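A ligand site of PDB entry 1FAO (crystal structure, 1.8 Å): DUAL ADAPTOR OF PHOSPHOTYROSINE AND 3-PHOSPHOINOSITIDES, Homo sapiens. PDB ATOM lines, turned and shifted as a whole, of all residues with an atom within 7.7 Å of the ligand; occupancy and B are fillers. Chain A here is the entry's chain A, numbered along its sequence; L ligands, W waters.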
ATOM      1  N   LYS A  26      24.040  20.944  -8.199  1.00  0.00           N
ATOM      2  CA  LYS A  26      22.708  20.576  -7.765  1.00  0.00           C
ATOM      3  C   LYS A  26      22.665  19.154  -7.253  1.00  0.00           C
ATOM      4  O   LYS A  26      23.427  18.299  -7.695  1.00  0.00           O
ATOM      5  CB  LYS A  26      21.716  20.723  -8.918  1.00  0.00           C
ATOM      6  CG  LYS A  26      22.104  19.966 -10.171  1.00  0.00           C
ATOM      7  CD  LYS A  26      20.934  19.859 -11.128  1.00  0.00           C
ATOM      8  CE  LYS A  26      19.940  18.822 -10.644  1.00  0.00           C
ATOM      9  NZ  LYS A  26      20.525  17.447 -10.675  1.00  0.00           N
ATOM     10  N   GLN A  27      21.752  18.915  -6.312  1.00  0.00           N
ATOM     11  CA  GLN A  27      21.588  17.598  -5.728  1.00  0.00           C
ATOM     12  C   GLN A  27      20.604  16.795  -6.567  1.00  0.00           C
ATOM     13  O   GLN A  27      19.682  17.351  -7.161  1.00  0.00           O
ATOM     14  CB  GLN A  27      21.044  17.738  -4.310  1.00  0.00           C
ATOM     15  CG  GLN A  27      20.901  16.430  -3.552  1.00  0.00           C
ATOM     16  CD  GLN A  27      20.466  16.630  -2.117  1.00  0.00           C
ATOM     17  OE1 GLN A  27      19.345  17.064  -1.856  1.00  0.00           O
ATOM     18  NE2 GLN A  27      21.355  16.330  -1.180  1.00  0.00           N
ATOM     19  N   GLY A  28      20.816  15.489  -6.621  1.00  0.00           N
ATOM     20  CA  GLY A  28      19.929  14.634  -7.383  1.00  0.00           C
ATOM     21  C   GLY A  28      18.634  14.426  -6.621  1.00  0.00           C
ATOM     22  O   GLY A  28      18.488  14.898  -5.485  1.00  0.00           O
ATOM     23  N   GLY A  29      17.704  13.697  -7.228  1.00  0.00           N
ATOM     24  CA  GLY A  29      16.417  13.431  -6.595  1.00  0.00           C
ATOM     25  C   GLY A  29      16.466  12.251  -5.647  1.00  0.00           C
ATOM     26  O   GLY A  29      16.604  12.432  -4.437  1.00  0.00           O
ATOM     27  N   LEU A  30      16.341  11.040  -6.200  1.00  0.00           N
ATOM     28  CA  LEU A  30      16.380   9.817  -5.399  1.00  0.00           C
ATOM     29  C   LEU A  30      17.827   9.588  -4.965  1.00  0.00           C
ATOM     30  O   LEU A  30      18.095   9.355  -3.791  1.00  0.00           O
ATOM     31  CB  LEU A  30      15.891   8.621  -6.220  1.00  0.00           C
ATOM     32  CG  LEU A  30      14.436   8.637  -6.668  1.00  0.00           C
ATOM     33  CD1 LEU A  30      14.144   7.394  -7.501  1.00  0.00           C
ATOM     34  CD2 LEU A  30      13.522   8.692  -5.451  1.00  0.00           C
ATOM     35  N   VAL A  31      18.736   9.642  -5.926  1.00  0.00           N
ATOM     36  CA  VAL A  31      20.156   9.490  -5.650  1.00  0.00           C
ATOM     37  C   VAL A  31      20.618  10.938  -5.494  1.00  0.00           C
ATOM     38  O   VAL A  31      20.723  11.682  -6.464  1.00  0.00           O
ATOM     39  CB  VAL A  31      20.894   8.831  -6.827  1.00  0.00           C
ATOM     40  CG1 VAL A  31      22.387   8.738  -6.517  1.00  0.00           C
ATOM     41  CG2 VAL A  31      20.315   7.450  -7.077  1.00  0.00           C
ATOM     42  N   LYS A  32      20.887  11.335  -4.251  1.00  0.00           N
ATOM     43  CA  LYS A  32      21.270  12.703  -3.943  1.00  0.00           C
ATOM     44  C   LYS A  32      22.715  13.115  -4.179  1.00  0.00           C
ATOM     45  O   LYS A  32      23.315  13.789  -3.345  1.00  0.00           O
ATOM     46  CB  LYS A  32      20.859  13.019  -2.504  1.00  0.00           C
ATOM     47  CG  LYS A  32      19.376  12.842  -2.258  1.00  0.00           C
ATOM     48  CD  LYS A  32      19.017  13.171  -0.827  1.00  0.00           C
ATOM     49  CE  LYS A  32      17.531  13.002  -0.577  1.00  0.00           C
ATOM     50  NZ  LYS A  32      17.179  13.339   0.825  1.00  0.00           N
ATOM     51  N   THR A  33      23.261  12.725  -5.325  1.00  0.00           N
ATOM     52  CA  THR A  33      24.623  13.106  -5.651  1.00  0.00           C
ATOM     53  C   THR A  33      24.607  14.558  -6.130  1.00  0.00           C
ATOM     54  O   THR A  33      23.604  15.027  -6.671  1.00  0.00           O
ATOM     55  CB  THR A  33      25.195  12.209  -6.763  1.00  0.00           C
ATOM     56  OG1 THR A  33      24.279  12.148  -7.856  1.00  0.00           O
ATOM     57  CG2 THR A  33      25.440  10.803  -6.223  1.00  0.00           C
ATOM     58  N   TRP A  34      25.708  15.269  -5.911  1.00  0.00           N
ATOM     59  CA  TRP A  34      25.788  16.661  -6.343  1.00  0.00           C
ATOM     60  C   TRP A  34      26.530  16.742  -7.666  1.00  0.00           C
ATOM     61  O   TRP A  34      27.645  16.251  -7.786  1.00  0.00           O
ATOM     62  CB  TRP A  34      26.481  17.512  -5.279  1.00  0.00           C
ATOM     63  CG  TRP A  34      25.619  17.757  -4.103  1.00  0.00           C
ATOM     64  CD1 TRP A  34      25.355  16.893  -3.076  1.00  0.00           C
ATOM     65  CD2 TRP A  34      24.831  18.921  -3.864  1.00  0.00           C
ATOM     66  NE1 TRP A  34      24.435  17.448  -2.213  1.00  0.00           N
ATOM     67  CE2 TRP A  34      24.098  18.700  -2.673  1.00  0.00           C
ATOM     68  CE3 TRP A  34      24.650  20.136  -4.537  1.00  0.00           C
ATOM     69  CZ2 TRP A  34      23.216  19.641  -2.147  1.00  0.00           C
ATOM     70  CZ3 TRP A  34      23.781  21.071  -4.013  1.00  0.00           C
ATOM     71  CH2 TRP A  34      23.069  20.814  -2.829  1.00  0.00           C
ATOM     72  N   LYS A  35      25.895  17.374  -8.646  1.00  0.00           N
ATOM     73  CA  LYS A  35      26.492  17.515  -9.965  1.00  0.00           C
ATOM     74  C   LYS A  35      26.513  18.961 -10.383  1.00  0.00           C
ATOM     75  O   LYS A  35      25.601  19.736 -10.059  1.00  0.00           O
ATOM     76  CB  LYS A  35      25.707  16.691 -10.990  1.00  0.00           C
ATOM     77  CG  LYS A  35      25.642  15.201 -10.677  1.00  0.00           C
ATOM     78  CD  LYS A  35      27.020  14.550 -10.798  1.00  0.00           C
ATOM     79  CE  LYS A  35      26.970  13.084 -10.408  1.00  0.00           C
ATOM     80  NZ  LYS A  35      28.312  12.432 -10.512  1.00  0.00           N
ATOM     81  N   THR A  36      27.564  19.342 -11.110  1.00  0.00           N
ATOM     82  CA  THR A  36      27.686  20.705 -11.588  1.00  0.00           C
ATOM     83  C   THR A  36      26.987  20.767 -12.942  1.00  0.00           C
ATOM     84  O   THR A  36      27.318  20.020 -13.865  1.00  0.00           O
ATOM     85  CB  THR A  36      29.146  21.109 -11.757  1.00  0.00           C
ATOM     86  OG1 THR A  36      29.857  20.815 -10.545  1.00  0.00           O
ATOM     87  CG2 THR A  36      29.260  22.597 -12.053  1.00  0.00           C
ATOM     88  N   ARG A  37      26.010  21.651 -13.033  1.00  0.00           N
ATOM     89  CA  ARG A  37      25.229  21.798 -14.250  1.00  0.00           C
ATOM     90  C   ARG A  37      25.165  23.242 -14.706  1.00  0.00           C
ATOM     91  O   ARG A  37      25.340  24.167 -13.908  1.00  0.00           O
ATOM     92  CB  ARG A  37      23.819  21.275 -14.007  1.00  0.00           C
ATOM     93  CG  ARG A  37      23.782  19.800 -13.656  1.00  0.00           C
ATOM     94  CD  ARG A  37      24.148  18.947 -14.865  1.00  0.00           C
ATOM     95  NE  ARG A  37      24.152  17.521 -14.549  1.00  0.00           N
ATOM     96  CZ  ARG A  37      25.253  16.775 -14.485  1.00  0.00           C
ATOM     97  NH1 ARG A  37      26.450  17.304 -14.697  1.00  0.00           N
ATOM     98  NH2 ARG A  37      25.154  15.477 -14.212  1.00  0.00           N
ATOM     99  N   PHE A  39      22.990  26.240 -15.877  1.00  0.00           N
ATOM    100  CA  PHE A  39      21.619  26.714 -15.782  1.00  0.00           C
ATOM    101  C   PHE A  39      21.407  27.943 -16.652  1.00  0.00           C
ATOM    102  O   PHE A  39      22.278  28.793 -16.783  1.00  0.00           O
ATOM    103  CB  PHE A  39      21.267  27.087 -14.335  1.00  0.00           C
ATOM    104  CG  PHE A  39      21.070  25.916 -13.429  1.00  0.00           C
ATOM    105  CD1 PHE A  39      22.158  25.150 -13.011  1.00  0.00           C
ATOM    106  CD2 PHE A  39      19.790  25.562 -13.002  1.00  0.00           C
ATOM    107  CE1 PHE A  39      21.966  24.048 -12.180  1.00  0.00           C
ATOM    108  CE2 PHE A  39      19.595  24.468 -12.167  1.00  0.00           C
ATOM    109  CZ  PHE A  39      20.685  23.708 -11.758  1.00  0.00           C
ATOM    110  N   TYR A  48      18.512  23.396 -17.130  1.00  0.00           N
ATOM    111  CA  TYR A  48      19.869  23.053 -16.733  1.00  0.00           C
ATOM    112  C   TYR A  48      20.345  21.975 -17.697  1.00  0.00           C
ATOM    113  O   TYR A  48      19.578  21.101 -18.123  1.00  0.00           O
ATOM    114  CB  TYR A  48      19.993  22.653 -15.256  1.00  0.00           C
ATOM    115  CG  TYR A  48      19.227  21.461 -14.765  1.00  0.00           C
ATOM    116  CD1 TYR A  48      19.717  20.168 -14.902  1.00  0.00           C
ATOM    117  CD2 TYR A  48      18.037  21.645 -14.064  1.00  0.00           C
ATOM    118  CE1 TYR A  48      19.047  19.076 -14.346  1.00  0.00           C
ATOM    119  CE2 TYR A  48      17.362  20.575 -13.508  1.00  0.00           C
ATOM    120  CZ  TYR A  48      17.868  19.300 -13.643  1.00  0.00           C
ATOM    121  OH  TYR A  48      17.172  18.274 -13.051  1.00  0.00           O
ATOM    122  N   PHE A  49      21.603  22.100 -18.079  1.00  0.00           N
ATOM    123  CA  PHE A  49      22.248  21.212 -19.044  1.00  0.00           C
ATOM    124  C   PHE A  49      23.458  20.547 -18.393  1.00  0.00           C
ATOM    125  O   PHE A  49      23.923  20.986 -17.344  1.00  0.00           O
ATOM    126  CB  PHE A  49      22.752  22.036 -20.239  1.00  0.00           C
ATOM    127  CG  PHE A  49      21.687  22.855 -20.928  1.00  0.00           C
ATOM    128  CD1 PHE A  49      21.119  23.959 -20.292  1.00  0.00           C
ATOM    129  CD2 PHE A  49      21.296  22.549 -22.227  1.00  0.00           C
ATOM    130  CE1 PHE A  49      20.168  24.759 -20.953  1.00  0.00           C
ATOM    131  CE2 PHE A  49      20.348  23.341 -22.892  1.00  0.00           C
ATOM    132  CZ  PHE A  49      19.792  24.439 -22.259  1.00  0.00           C
ATOM    133  N   LYS A  50      23.961  19.487 -19.023  1.00  0.00           N
ATOM    134  CA  LYS A  50      25.136  18.803 -18.495  1.00  0.00           C
ATOM    135  C   LYS A  50      26.243  19.842 -18.381  1.00  0.00           C
ATOM    136  O   LYS A  50      26.945  19.908 -17.363  1.00  0.00           O
ATOM    137  CB  LYS A  50      25.585  17.676 -19.435  1.00  0.00           C
ATOM    138  CG  LYS A  50      24.662  16.481 -19.465  1.00  0.00           C
ATOM    139  CD  LYS A  50      24.516  15.856 -18.084  1.00  0.00           C
ATOM    140  CE  LYS A  50      23.619  14.622 -18.134  1.00  0.00           C
ATOM    141  NZ  LYS A  50      23.286  14.094 -16.780  1.00  0.00           N
ATOM    142  N   ILE A  58      18.695  18.984 -19.688  1.00  0.00           N
ATOM    143  CA  ILE A  58      18.342  17.763 -18.977  1.00  0.00           C
ATOM    144  C   ILE A  58      16.899  17.944 -18.540  1.00  0.00           C
ATOM    145  O   ILE A  58      16.098  17.011 -18.580  1.00  0.00           O
ATOM    146  CB  ILE A  58      19.209  17.598 -17.711  1.00  0.00           C
ATOM    147  CG1 ILE A  58      20.641  17.247 -18.113  1.00  0.00           C
ATOM    148  CG2 ILE A  58      18.619  16.519 -16.817  1.00  0.00           C
ATOM    149  CD1 ILE A  58      21.613  17.307 -16.953  1.00  0.00           C
ATOM    150  N   ARG A  59      16.574  19.172 -18.147  1.00  0.00           N
ATOM    151  CA  ARG A  59      15.233  19.480 -17.688  1.00  0.00           C
ATOM    152  C   ARG A  59      14.885  20.937 -17.916  1.00  0.00           C
ATOM    153  O   ARG A  59      15.749  21.807 -17.893  1.00  0.00           O
ATOM    154  CB  ARG A  59      15.129  19.128 -16.203  1.00  0.00           C
ATOM    155  CG  ARG A  59      13.713  19.068 -15.662  1.00  0.00           C
ATOM    156  CD  ARG A  59      13.665  18.276 -14.370  1.00  0.00           C
ATOM    157  NE  ARG A  59      12.305  18.071 -13.899  1.00  0.00           N
ATOM    158  CZ  ARG A  59      11.969  17.223 -12.932  1.00  0.00           C
ATOM    159  NH1 ARG A  59      12.895  16.507 -12.329  1.00  0.00           N
ATOM    160  NH2 ARG A  59      10.701  17.114 -12.565  1.00  0.00           N
ATOM    161  N   ARG A  88       8.865  18.614  -6.455  1.00  0.00           N
ATOM    162  CA  ARG A  88      10.212  18.481  -5.941  1.00  0.00           C
ATOM    163  C   ARG A  88      10.826  19.811  -5.551  1.00  0.00           C
ATOM    164  O   ARG A  88      10.462  20.860  -6.081  1.00  0.00           O
ATOM    165  CB  ARG A  88      11.096  17.827  -7.000  1.00  0.00           C
ATOM    166  CG  ARG A  88      12.583  17.814  -6.664  1.00  0.00           C
ATOM    167  CD  ARG A  88      13.347  17.075  -7.721  1.00  0.00           C
ATOM    168  NE  ARG A  88      14.791  17.148  -7.527  1.00  0.00           N
ATOM    169  CZ  ARG A  88      15.668  16.609  -8.363  1.00  0.00           C
ATOM    170  NH1 ARG A  88      15.241  15.959  -9.441  1.00  0.00           N
ATOM    171  NH2 ARG A  88      16.970  16.738  -8.131  1.00  0.00           N
ATOM    172  N   PHE A  90      14.382  21.663  -5.448  1.00  0.00           N
ATOM    173  CA  PHE A  90      15.722  21.548  -5.989  1.00  0.00           C
ATOM    174  C   PHE A  90      16.695  22.248  -5.062  1.00  0.00           C
ATOM    175  O   PHE A  90      16.431  23.346  -4.587  1.00  0.00           O
ATOM    176  CB  PHE A  90      15.802  22.153  -7.381  1.00  0.00           C
ATOM    177  CG  PHE A  90      15.029  21.373  -8.412  1.00  0.00           C
ATOM    178  CD1 PHE A  90      13.652  21.497  -8.521  1.00  0.00           C
ATOM    179  CD2 PHE A  90      15.703  20.492  -9.262  1.00  0.00           C
ATOM    180  CE1 PHE A  90      12.939  20.748  -9.454  1.00  0.00           C
ATOM    181  CE2 PHE A  90      14.993  19.734 -10.199  1.00  0.00           C
ATOM    182  CZ  PHE A  90      13.612  19.862 -10.295  1.00  0.00           C
HETATM  183  C1  LIG L   1      21.854  11.261 -10.648  1.00  0.00           C
HETATM  184  O1  LIG L   1      22.908  10.663  -9.883  1.00  0.00           O
HETATM  185  C2  LIG L   1      22.150  12.741 -10.863  1.00  0.00           C
HETATM  186  O2  LIG L   1      22.232  13.409  -9.610  1.00  0.00           O
HETATM  187  C3  LIG L   1      21.058  13.364 -11.701  1.00  0.00           C
HETATM  188  O3  LIG L   1      21.359  14.736 -11.959  1.00  0.00           O
HETATM  189  C4  LIG L   1      19.687  13.254 -11.018  1.00  0.00           C
HETATM  190  O4  LIG L   1      18.662  13.730 -11.890  1.00  0.00           O
HETATM  191  C5  LIG L   1      19.355  11.827 -10.574  1.00  0.00           C
HETATM  192  O5  LIG L   1      18.246  11.867  -9.667  1.00  0.00           O
HETATM  193  C6  LIG L   1      20.517  11.062  -9.933  1.00  0.00           C
HETATM  194  O6  LIG L   1      20.222   9.677  -9.907  1.00  0.00           O
HETATM  195  P1  LIG L   1      24.169   9.934 -10.602  1.00  0.00           P
HETATM  196  O7  LIG L   1      25.242   9.865  -9.531  1.00  0.00           O
HETATM  197  O8  LIG L   1      24.528  10.814 -11.783  1.00  0.00           O
HETATM  198  O9  LIG L   1      23.681   8.563 -11.022  1.00  0.00           O
HETATM  199  P2  LIG L   1      21.531  15.262 -13.491  1.00  0.00           P
HETATM  200  O10 LIG L   1      21.838  16.747 -13.383  1.00  0.00           O
HETATM  201  O11 LIG L   1      22.640  14.432 -14.117  1.00  0.00           O
HETATM  202  O12 LIG L   1      20.178  15.006 -14.140  1.00  0.00           O
HETATM  203  P3  LIG L   1      17.960  15.179 -11.664  1.00  0.00           P
HETATM  204  O13 LIG L   1      18.501  15.753 -10.367  1.00  0.00           O
HETATM  205  O14 LIG L   1      18.351  16.002 -12.875  1.00  0.00           O
HETATM  206  O15 LIG L   1      16.452  14.923 -11.601  1.00  0.00           O
HETATM  207  P4  LIG L   1      17.116  10.688  -9.657  1.00  0.00           P
HETATM  208  O16 LIG L   1      15.932  11.317  -8.942  1.00  0.00           O
HETATM  209  O17 LIG L   1      16.837  10.370 -11.114  1.00  0.00           O
HETATM  210  O18 LIG L   1      17.757   9.535  -8.892  1.00  0.00           O
HETATM  211  O   HOH W   1      17.489   6.986  -9.026  1.00  0.00           O
HETATM  212  O   HOH W   2      27.031  10.221 -13.021  1.00  0.00           O
HETATM  213  O   HOH W   3      27.768   9.955  -9.432  1.00  0.00           O
HETATM  214  O   HOH W   4      22.584  16.265  -9.357  1.00  0.00           O
HETATM  215  O   HOH W   5      23.599  11.879 -14.053  1.00  0.00           O
HETATM  216  O   HOH W   6      21.870   7.100 -10.280  1.00  0.00           O
HETATM  217  O   HOH W   7      25.637   7.627  -7.873  1.00  0.00           O
HETATM  218  O   HOH W   8      15.877  15.814 -14.757  1.00  0.00           O
HETATM  219  O   HOH W   9      19.194  12.852 -15.364  1.00  0.00           O
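Residues that only touch the ligand: Gly 28 (3.4 Å), Ile 58 (3.4 Å), Lys 35 (3.6 Å) and Gln 27 (3.8 Å).
Water W3 bridges an oxygen (O7) of the ligand (2.5 Å) and the side-chain amino group (NZ) of Lys 35 (2.8 Å). Water W4 lies within hydrogen-bond range of the side-chain amino group (NZ) of Lys 26 (2.7 Å), an oxygen (O2) of the ligand (2.9 Å), the backbone carbonyl oxygen (O) of Thr 33 (3.1 Å) and the backbone NH (N) of Gly 28 (3.3 Å). Water W8 bridges O14 of the ligand (3.1 Å) and OH of Tyr 48 (3.3 Å).
The backbone NH of Lys 26 is in hydrogen-bond range of the backbone carbonyl oxygen of Lys 35, 2.7 Å away. NE1 of Trp 34 lies close to NE2 of Gln 27, at 3.4 Å. N of Tyr 48 lies within hydrogen-bond range of O of Arg 59 (3.3 Å). The guanidinium group (NH2) of Arg 88 sits at hydrogen-bond distance from the backbone carbonyl oxygen (O) of Gln 27 (2.9 Å). The backbone carbonyl oxygen of Tyr 48 lies within hydrogen-bond range of the backbone NH of Ile 58 (2.8 Å). O of Thr 33 sits at hydrogen-bond distance from N of Gly 28, at 2.8 Å.
The side-chain hydroxyl (OH) of Tyr 48 lies within hydrogen-bond range of an oxygen (O14) of the ligand. The backbone NH (N) of Val 31 is in hydrogen-bond range of an oxygen (O18) of the ligand, at 3.1 Å. An oxygen (O15) of the ligand is in salt-bridge range of the guanidinium group of Arg 59, at 3.96 Å. The guanidinium group (NE) of Arg 37 lies within salt-bridge range of an oxygen (O10) of the ligand. An oxygen (O15) of the ligand lies within salt-bridge range of the guanidinium group of Arg 88, at 2.7 Å. The side-chain amino group (NZ) of Lys 50 is in salt-bridge range of an oxygen (O11) of the ligand, 2.8 Å away. N of Leu 30 lies within hydrogen-bond range of O16 of the ligand (2.8 Å). O1 of the ligand lies within hydrogen-bond range of OG1 of Thr 33 (2.9 Å). The backbone NH of Gly 29 sits at hydrogen-bond distance from an oxygen (O5) of the ligand. NZ of Lys 26 lies within salt-bridge range of O13 of the ligand, 2.7 Å away.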
